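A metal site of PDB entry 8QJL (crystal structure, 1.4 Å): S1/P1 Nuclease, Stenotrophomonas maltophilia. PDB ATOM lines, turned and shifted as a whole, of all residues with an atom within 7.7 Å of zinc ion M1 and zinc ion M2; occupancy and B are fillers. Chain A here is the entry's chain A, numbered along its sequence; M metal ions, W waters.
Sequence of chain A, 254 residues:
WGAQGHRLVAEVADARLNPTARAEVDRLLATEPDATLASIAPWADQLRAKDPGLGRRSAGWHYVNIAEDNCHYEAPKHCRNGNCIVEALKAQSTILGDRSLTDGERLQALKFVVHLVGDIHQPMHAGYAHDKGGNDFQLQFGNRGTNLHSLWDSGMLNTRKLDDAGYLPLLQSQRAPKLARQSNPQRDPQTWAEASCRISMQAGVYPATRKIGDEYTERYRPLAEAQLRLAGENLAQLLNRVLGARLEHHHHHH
A ring nitrogen (ND1) of His 6 sits at hydrogen-bond distance from a ring nitrogen (ND1) of His 115, at 3.5 Å. O of His 62 lies within hydrogen-bond range of ND1 of His 125 (2.7 Å). A ring nitrogen (ND1) of His 115 sits at hydrogen-bond distance from the backbone carbonyl oxygen (O) of Ala 41 (2.7 Å). The indole nitrogen (NE1) of Trp 1 lies within hydrogen-bond range of the backbone carbonyl oxygen (O) of Gly 118.
Five residues have an atom within 4 Å of zinc ion M1: Trp 1, His 6, Asp 45, His 115 and Asp 119. The nearest printed residue that does not touch zinc ion M1 is His 125 (4.2 Å).
Within 4 Å of zinc ion M2: Asp 45, His 62, His 115 and Asp 119.
Zinc ion M2 is bound by water W2 (2.0 Å), a ring nitrogen (ND1) of His 62 (2.0 Å), the side-chain carboxylate of Asp 119 (2.1 Å), a ring nitrogen (NE2) of His 115 (2.1 Å), the side-chain carboxylate of Asp 45 (2.5 Å) and water W1 (2.5 Å). Zinc ion M2 has six donor atoms within binding distance.
Zinc ion M1 is bound by water W2 (1.9 Å), a ring nitrogen (NE2) of His 6 (2.0 Å), the side-chain carboxylate (OD1) of Asp 119 (2.1 Å), the backbone nitrogen (N) of Trp 1 (2.1 Å) and the backbone carbonyl oxygen (O) of Trp 1 (2.3 Å). Zinc ion M1 has five donor atoms within binding distance.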
ATOM      1  N   TRP A   1      -9.797  25.573   8.406  1.00  0.00           N
ATOM      2  CA  TRP A   1     -10.394  25.539   7.053  1.00  0.00           C
ATOM      3  C   TRP A   1      -9.966  24.249   6.348  1.00  0.00           C
ATOM      4  O   TRP A   1      -8.940  23.658   6.687  1.00  0.00           O
ATOM      5  CB  TRP A   1      -9.897  26.702   6.222  1.00  0.00           C
ATOM      6  CG  TRP A   1     -10.097  28.037   6.852  1.00  0.00           C
ATOM      7  CD1 TRP A   1      -9.130  28.762   7.490  1.00  0.00           C
ATOM      8  CD2 TRP A   1     -11.300  28.812   6.930  1.00  0.00           C
ATOM      9  NE1 TRP A   1      -9.648  29.943   7.948  1.00  0.00           N
ATOM     10  CE2 TRP A   1     -10.961  30.008   7.588  1.00  0.00           C
ATOM     11  CE3 TRP A   1     -12.615  28.623   6.507  1.00  0.00           C
ATOM     12  CZ2 TRP A   1     -11.896  31.009   7.858  1.00  0.00           C
ATOM     13  CZ3 TRP A   1     -13.532  29.626   6.768  1.00  0.00           C
ATOM     14  CH2 TRP A   1     -13.183  30.800   7.423  1.00  0.00           C
ATOM     15  N   GLY A   2     -10.735  23.871   5.346  1.00  0.00           N
ATOM     16  CA  GLY A   2     -10.245  22.920   4.338  1.00  0.00           C
ATOM     17  C   GLY A   2      -9.195  23.531   3.437  1.00  0.00           C
ATOM     18  O   GLY A   2      -8.791  24.707   3.600  1.00  0.00           O
ATOM     19  N   ALA A   3      -8.706  22.732   2.514  1.00  0.00           N
ATOM     20  CA  ALA A   3      -7.513  23.096   1.738  1.00  0.00           C
ATOM     21  C   ALA A   3      -7.784  24.351   0.929  1.00  0.00           C
ATOM     22  O   ALA A   3      -6.920  25.234   0.910  1.00  0.00           O
ATOM     23  CB  ALA A   3      -7.072  21.932   0.905  1.00  0.00           C
ATOM     24  N   GLY A   5      -9.769  26.893   1.506  1.00  0.00           N
ATOM     25  CA  GLY A   5      -9.709  28.055   2.382  1.00  0.00           C
ATOM     26  C   GLY A   5      -8.276  28.416   2.732  1.00  0.00           C
ATOM     27  O   GLY A   5      -7.919  29.612   2.663  1.00  0.00           O
ATOM     28  N   HIS A   6      -7.438  27.429   3.046  1.00  0.00           N
ATOM     29  CA  HIS A   6      -6.011  27.690   3.348  1.00  0.00           C
ATOM     30  C   HIS A   6      -5.296  28.320   2.146  1.00  0.00           C
ATOM     31  O   HIS A   6      -4.526  29.277   2.343  1.00  0.00           O
ATOM     32  CB  HIS A   6      -5.312  26.437   3.830  1.00  0.00           C
ATOM     33  CG  HIS A   6      -5.658  26.165   5.244  1.00  0.00           C
ATOM     34  ND1 HIS A   6      -5.207  26.971   6.268  1.00  0.00           N
ATOM     35  CD2 HIS A   6      -6.495  25.257   5.798  1.00  0.00           C
ATOM     36  CE1 HIS A   6      -5.776  26.567   7.416  1.00  0.00           C
ATOM     37  NE2 HIS A   6      -6.563  25.497   7.148  1.00  0.00           N
ATOM     38  N   ALA A  41       0.039  25.874   1.869  1.00  0.00           N
ATOM     39  CA  ALA A  41      -0.927  26.337   2.893  1.00  0.00           C
ATOM     40  C   ALA A  41      -1.686  25.171   3.532  1.00  0.00           C
ATOM     41  O   ALA A  41      -1.966  25.237   4.738  1.00  0.00           O
ATOM     42  CB  ALA A  41      -1.857  27.396   2.333  1.00  0.00           C
ATOM     43  N   PRO A  42      -2.110  24.125   2.799  1.00  0.00           N
ATOM     44  CA  PRO A  42      -2.773  22.959   3.407  1.00  0.00           C
ATOM     45  C   PRO A  42      -1.867  21.927   4.053  1.00  0.00           C
ATOM     46  O   PRO A  42      -2.374  20.990   4.687  1.00  0.00           O
ATOM     47  CB  PRO A  42      -3.486  22.301   2.214  1.00  0.00           C
ATOM     48  CG  PRO A  42      -3.536  23.363   1.154  1.00  0.00           C
ATOM     49  CD  PRO A  42      -2.210  24.049   1.330  1.00  0.00           C
ATOM     50  N   ALA A  44      -0.054  21.451   6.641  1.00  0.00           N
ATOM     51  CA  ALA A  44      -0.112  21.060   8.065  1.00  0.00           C
ATOM     52  C   ALA A  44      -1.295  20.127   8.330  1.00  0.00           C
ATOM     53  O   ALA A  44      -1.282  19.443   9.378  1.00  0.00           O
ATOM     54  CB  ALA A  44      -0.174  22.255   8.974  1.00  0.00           C
ATOM     55  N   ASP A  45      -2.298  20.067   7.429  1.00  0.00           N
ATOM     56  CA  ASP A  45      -3.432  19.131   7.593  1.00  0.00           C
ATOM     57  C   ASP A  45      -3.192  17.795   6.891  1.00  0.00           C
ATOM     58  O   ASP A  45      -4.056  16.898   7.014  1.00  0.00           O
ATOM     59  CB  ASP A  45      -4.715  19.721   6.986  1.00  0.00           C
ATOM     60  CG  ASP A  45      -5.449  20.763   7.828  1.00  0.00           C
ATOM     61  OD1 ASP A  45      -5.091  20.936   9.030  1.00  0.00           O
ATOM     62  OD2 ASP A  45      -6.369  21.441   7.231  1.00  0.00           O
ATOM     63  N   GLN A  46      -2.097  17.673   6.136  1.00  0.00           N
ATOM     64  CA  GLN A  46      -1.895  16.574   5.184  1.00  0.00           C
ATOM     65  C   GLN A  46      -0.694  15.734   5.581  1.00  0.00           C
ATOM     66  O   GLN A  46      -0.239  14.935   4.763  1.00  0.00           O
ATOM     67  CB  GLN A  46      -1.742  17.162   3.774  1.00  0.00           C
ATOM     68  CG  GLN A  46      -2.996  17.887   3.326  1.00  0.00           C
ATOM     69  CD  GLN A  46      -2.993  18.454   1.931  1.00  0.00           C
ATOM     70  OE1 GLN A  46      -1.945  18.603   1.297  1.00  0.00           O
ATOM     71  NE2 GLN A  46      -4.175  18.810   1.454  1.00  0.00           N
ATOM     72  N   SER A  58       1.612  17.735  16.131  1.00  0.00           N
ATOM     73  CA  SER A  58       1.128  19.117  15.858  1.00  0.00           C
ATOM     74  C   SER A  58      -0.389  19.215  15.652  1.00  0.00           C
ATOM     75  O   SER A  58      -0.869  20.301  15.406  1.00  0.00           O
ATOM     76  CB  SER A  58       1.864  19.703  14.687  1.00  0.00           C
ATOM     77  OG  SER A  58       1.658  18.981  13.497  1.00  0.00           O
ATOM     78  N   ALA A  59      -1.146  18.129  15.798  1.00  0.00           N
ATOM     79  CA  ALA A  59      -2.593  18.165  15.503  1.00  0.00           C
ATOM     80  C   ALA A  59      -3.332  19.162  16.414  1.00  0.00           C
ATOM     81  O   ALA A  59      -4.254  19.882  15.946  1.00  0.00           O
ATOM     82  CB  ALA A  59      -3.219  16.814  15.579  1.00  0.00           C
ATOM     83  N   TRP A  61      -2.252  21.910  17.497  1.00  0.00           N
ATOM     84  CA  TRP A  61      -1.817  23.306  17.219  1.00  0.00           C
ATOM     85  C   TRP A  61      -2.859  24.032  16.359  1.00  0.00           C
ATOM     86  O   TRP A  61      -2.703  25.216  16.167  1.00  0.00           O
ATOM     87  CB  TRP A  61      -0.470  23.324  16.510  1.00  0.00           C
ATOM     88  CG  TRP A  61       0.654  22.697  17.241  1.00  0.00           C
ATOM     89  CD1 TRP A  61       0.688  22.122  18.490  1.00  0.00           C
ATOM     90  CD2 TRP A  61       1.999  22.650  16.751  1.00  0.00           C
ATOM     91  NE1 TRP A  61       1.951  21.721  18.794  1.00  0.00           N
ATOM     92  CE2 TRP A  61       2.774  21.983  17.737  1.00  0.00           C
ATOM     93  CE3 TRP A  61       2.618  23.081  15.572  1.00  0.00           C
ATOM     94  CZ2 TRP A  61       4.137  21.772  17.573  1.00  0.00           C
ATOM     95  CZ3 TRP A  61       3.959  22.830  15.405  1.00  0.00           C
ATOM     96  CH2 TRP A  61       4.710  22.197  16.394  1.00  0.00           C
ATOM     97  N   HIS A  62      -3.861  23.324  15.808  1.00  0.00           N
ATOM     98  CA  HIS A  62      -4.800  23.946  14.849  1.00  0.00           C
ATOM     99  C   HIS A  62      -5.966  24.659  15.538  1.00  0.00           C
ATOM    100  O   HIS A  62      -6.722  25.312  14.839  1.00  0.00           O
ATOM    101  CB  HIS A  62      -5.306  22.917  13.840  1.00  0.00           C
ATOM    102  CG  HIS A  62      -4.237  22.315  13.008  1.00  0.00           C
ATOM    103  ND1 HIS A  62      -4.283  22.305  11.607  1.00  0.00           N
ATOM    104  CD2 HIS A  62      -3.122  21.652  13.377  1.00  0.00           C
ATOM    105  CE1 HIS A  62      -3.207  21.639  11.182  1.00  0.00           C
ATOM    106  NE2 HIS A  62      -2.485  21.251  12.236  1.00  0.00           N
ATOM    107  N   TYR A  63      -6.093  24.587  16.858  1.00  0.00           N
ATOM    108  CA  TYR A  63      -7.286  25.154  17.517  1.00  0.00           C
ATOM    109  C   TYR A  63      -6.976  25.516  18.956  1.00  0.00           C
ATOM    110  O   TYR A  63      -5.893  25.216  19.487  1.00  0.00           O
ATOM    111  CB  TYR A  63      -8.467  24.213  17.426  1.00  0.00           C
ATOM    112  CG  TYR A  63      -8.207  22.865  18.009  1.00  0.00           C
ATOM    113  CD1 TYR A  63      -7.627  21.856  17.244  1.00  0.00           C
ATOM    114  CD2 TYR A  63      -8.482  22.622  19.347  1.00  0.00           C
ATOM    115  CE1 TYR A  63      -7.343  20.633  17.827  1.00  0.00           C
ATOM    116  CE2 TYR A  63      -8.231  21.382  19.929  1.00  0.00           C
ATOM    117  CZ  TYR A  63      -7.663  20.393  19.167  1.00  0.00           C
ATOM    118  OH  TYR A  63      -7.407  19.166  19.739  1.00  0.00           O
ATOM    119  N   ILE A  85      -3.253  26.634  19.230  1.00  0.00           N
ATOM    120  CA  ILE A  85      -2.867  27.481  18.082  1.00  0.00           C
ATOM    121  C   ILE A  85      -2.212  28.769  18.560  1.00  0.00           C
ATOM    122  O   ILE A  85      -1.407  29.312  17.807  1.00  0.00           O
ATOM    123  CB  ILE A  85      -4.082  27.726  17.190  1.00  0.00           C
ATOM    124  CG1 ILE A  85      -3.664  28.326  15.852  1.00  0.00           C
ATOM    125  CG2 ILE A  85      -5.167  28.549  17.876  1.00  0.00           C
ATOM    126  CD1 ILE A  85      -4.691  28.102  14.754  1.00  0.00           C
ATOM    127  N   HIS A 115      -0.434  28.168   7.559  1.00  0.00           N
ATOM    128  CA  HIS A 115      -1.619  27.384   7.885  1.00  0.00           C
ATOM    129  C   HIS A 115      -2.326  27.981   9.094  1.00  0.00           C
ATOM    130  O   HIS A 115      -3.555  28.101   9.110  1.00  0.00           O
ATOM    131  CB  HIS A 115      -1.249  25.941   8.149  1.00  0.00           C
ATOM    132  CG  HIS A 115      -2.436  25.058   8.267  1.00  0.00           C
ATOM    133  ND1 HIS A 115      -2.997  24.452   7.154  1.00  0.00           N
ATOM    134  CD2 HIS A 115      -3.143  24.658   9.349  1.00  0.00           C
ATOM    135  CE1 HIS A 115      -4.038  23.720   7.564  1.00  0.00           C
ATOM    136  NE2 HIS A 115      -4.149  23.824   8.921  1.00  0.00           N
ATOM    137  N   LEU A 116      -1.565  28.226  10.145  1.00  0.00           N
ATOM    138  CA  LEU A 116      -2.134  28.569  11.468  1.00  0.00           C
ATOM    139  C   LEU A 116      -2.727  29.993  11.420  1.00  0.00           C
ATOM    140  O   LEU A 116      -3.720  30.244  12.107  1.00  0.00           O
ATOM    141  CB  LEU A 116      -1.089  28.420  12.567  1.00  0.00           C
ATOM    142  CG  LEU A 116      -0.629  26.980  12.830  1.00  0.00           C
ATOM    143  CD1 LEU A 116       0.346  27.000  13.950  1.00  0.00           C
ATOM    144  CD2 LEU A 116      -1.775  26.044  13.122  1.00  0.00           C
ATOM    145  N   GLY A 118      -4.329  31.027   8.968  1.00  0.00           N
ATOM    146  CA  GLY A 118      -5.649  30.646   8.424  1.00  0.00           C
ATOM    147  C   GLY A 118      -6.563  30.073   9.519  1.00  0.00           C
ATOM    148  O   GLY A 118      -7.642  30.607   9.771  1.00  0.00           O
ATOM    149  N   ASP A 119      -6.095  29.036  10.217  1.00  0.00           N
ATOM    150  CA  ASP A 119      -6.963  28.350  11.192  1.00  0.00           C
ATOM    151  C   ASP A 119      -7.375  29.277  12.340  1.00  0.00           C
ATOM    152  O   ASP A 119      -8.510  29.134  12.855  1.00  0.00           O
ATOM    153  CB  ASP A 119      -6.327  27.094  11.768  1.00  0.00           C
ATOM    154  CG  ASP A 119      -6.544  25.859  10.905  1.00  0.00           C
ATOM    155  OD1 ASP A 119      -7.337  25.918   9.967  1.00  0.00           O
ATOM    156  OD2 ASP A 119      -5.874  24.806  11.214  1.00  0.00           O
ATOM    157  N   ILE A 120      -6.549  30.225  12.769  1.00  0.00           N
ATOM    158  CA  ILE A 120      -6.865  31.044  13.954  1.00  0.00           C
ATOM    159  C   ILE A 120      -7.940  32.067  13.607  1.00  0.00           C
ATOM    160  O   ILE A 120      -8.473  32.670  14.526  1.00  0.00           O
ATOM    161  CB  ILE A 120      -5.585  31.685  14.527  1.00  0.00           C
ATOM    162  CG1 ILE A 120      -5.722  32.040  15.998  1.00  0.00           C
ATOM    163  CG2 ILE A 120      -5.093  32.869  13.731  1.00  0.00           C
ATOM    164  CD1 ILE A 120      -4.387  32.349  16.688  1.00  0.00           C
ATOM    165  N   GLN A 122     -10.612  30.966  11.709  1.00  0.00           N
ATOM    166  CA  GLN A 122     -11.817  30.130  11.503  1.00  0.00           C
ATOM    167  C   GLN A 122     -12.531  30.122  12.842  1.00  0.00           C
ATOM    168  O   GLN A 122     -12.008  29.525  13.792  1.00  0.00           O
ATOM    169  CB  GLN A 122     -11.406  28.737  11.046  1.00  0.00           C
ATOM    170  CG  GLN A 122     -12.411  27.958  10.202  1.00  0.00           C
ATOM    171  CD  GLN A 122     -13.678  27.515  10.892  1.00  0.00           C
ATOM    172  OE1 GLN A 122     -14.382  28.308  11.521  1.00  0.00           O
ATOM    173  NE2 GLN A 122     -13.989  26.221  10.800  1.00  0.00           N
ATOM    174  N   HIS A 125     -12.514  27.039  15.090  1.00  0.00           N
ATOM    175  CA  HIS A 125     -11.195  26.635  15.604  1.00  0.00           C
ATOM    176  C   HIS A 125     -10.877  27.367  16.918  1.00  0.00           C
ATOM    177  O   HIS A 125      -9.784  27.079  17.472  1.00  0.00           O
ATOM    178  CB  HIS A 125     -10.096  26.851  14.567  1.00  0.00           C
ATOM    179  CG  HIS A 125     -10.026  25.787  13.522  1.00  0.00           C
ATOM    180  ND1 HIS A 125      -8.904  25.017  13.358  1.00  0.00           N
ATOM    181  CD2 HIS A 125     -10.972  25.311  12.643  1.00  0.00           C
ATOM    182  CE1 HIS A 125      -9.148  24.111  12.409  1.00  0.00           C
ATOM    183  NE2 HIS A 125     -10.424  24.238  11.980  1.00  0.00           N
ATOM    184  N   HIS A 149     -18.747  22.581  12.656  1.00  0.00           N
ATOM    185  CA  HIS A 149     -17.301  22.771  12.409  1.00  0.00           C
ATOM    186  C   HIS A 149     -17.020  22.657  10.903  1.00  0.00           C
ATOM    187  O   HIS A 149     -16.449  23.586  10.302  1.00  0.00           O
ATOM    188  CB  HIS A 149     -16.472  21.788  13.216  1.00  0.00           C
ATOM    189  CG  HIS A 149     -15.020  22.107  13.150  1.00  0.00           C
ATOM    190  ND1 HIS A 149     -14.360  22.837  14.085  1.00  0.00           N
ATOM    191  CD2 HIS A 149     -14.179  21.922  12.124  1.00  0.00           C
ATOM    192  CE1 HIS A 149     -13.104  23.034  13.657  1.00  0.00           C
ATOM    193  NE2 HIS A 149     -12.981  22.503  12.428  1.00  0.00           N
ATOM    194  N   ASP A 153     -15.548  25.090   8.026  1.00  0.00           N
ATOM    195  CA  ASP A 153     -14.269  24.730   7.388  1.00  0.00           C
ATOM    196  C   ASP A 153     -14.403  24.758   5.870  1.00  0.00           C
ATOM    197  O   ASP A 153     -13.427  25.190   5.208  1.00  0.00           O
ATOM    198  CB  ASP A 153     -13.742  23.354   7.785  1.00  0.00           C
ATOM    199  CG  ASP A 153     -12.823  23.294   9.003  1.00  0.00           C
ATOM    200  OD1 ASP A 153     -12.363  24.336   9.483  1.00  0.00           O
ATOM    201  OD2 ASP A 153     -12.626  22.152   9.497  1.00  0.00           O
HETATM  202 ZN    ZN M   1      -7.874  24.641   8.417  1.00  0.00          ZN
HETATM  203 ZN    ZN M   2      -5.588  23.019  10.234  1.00  0.00          ZN
HETATM  204 ZN    ZN M   3     -11.392  22.622  11.062  1.00  0.00          ZN
HETATM  205  O   HOH W   1      -7.111  21.517  11.563  1.00  0.00           O
HETATM  206  O   HOH W   2      -7.264  22.987   9.203  1.00  0.00           O
HETATM  207  O   HOH W   3      -9.854  22.410   9.655  1.00  0.00           O
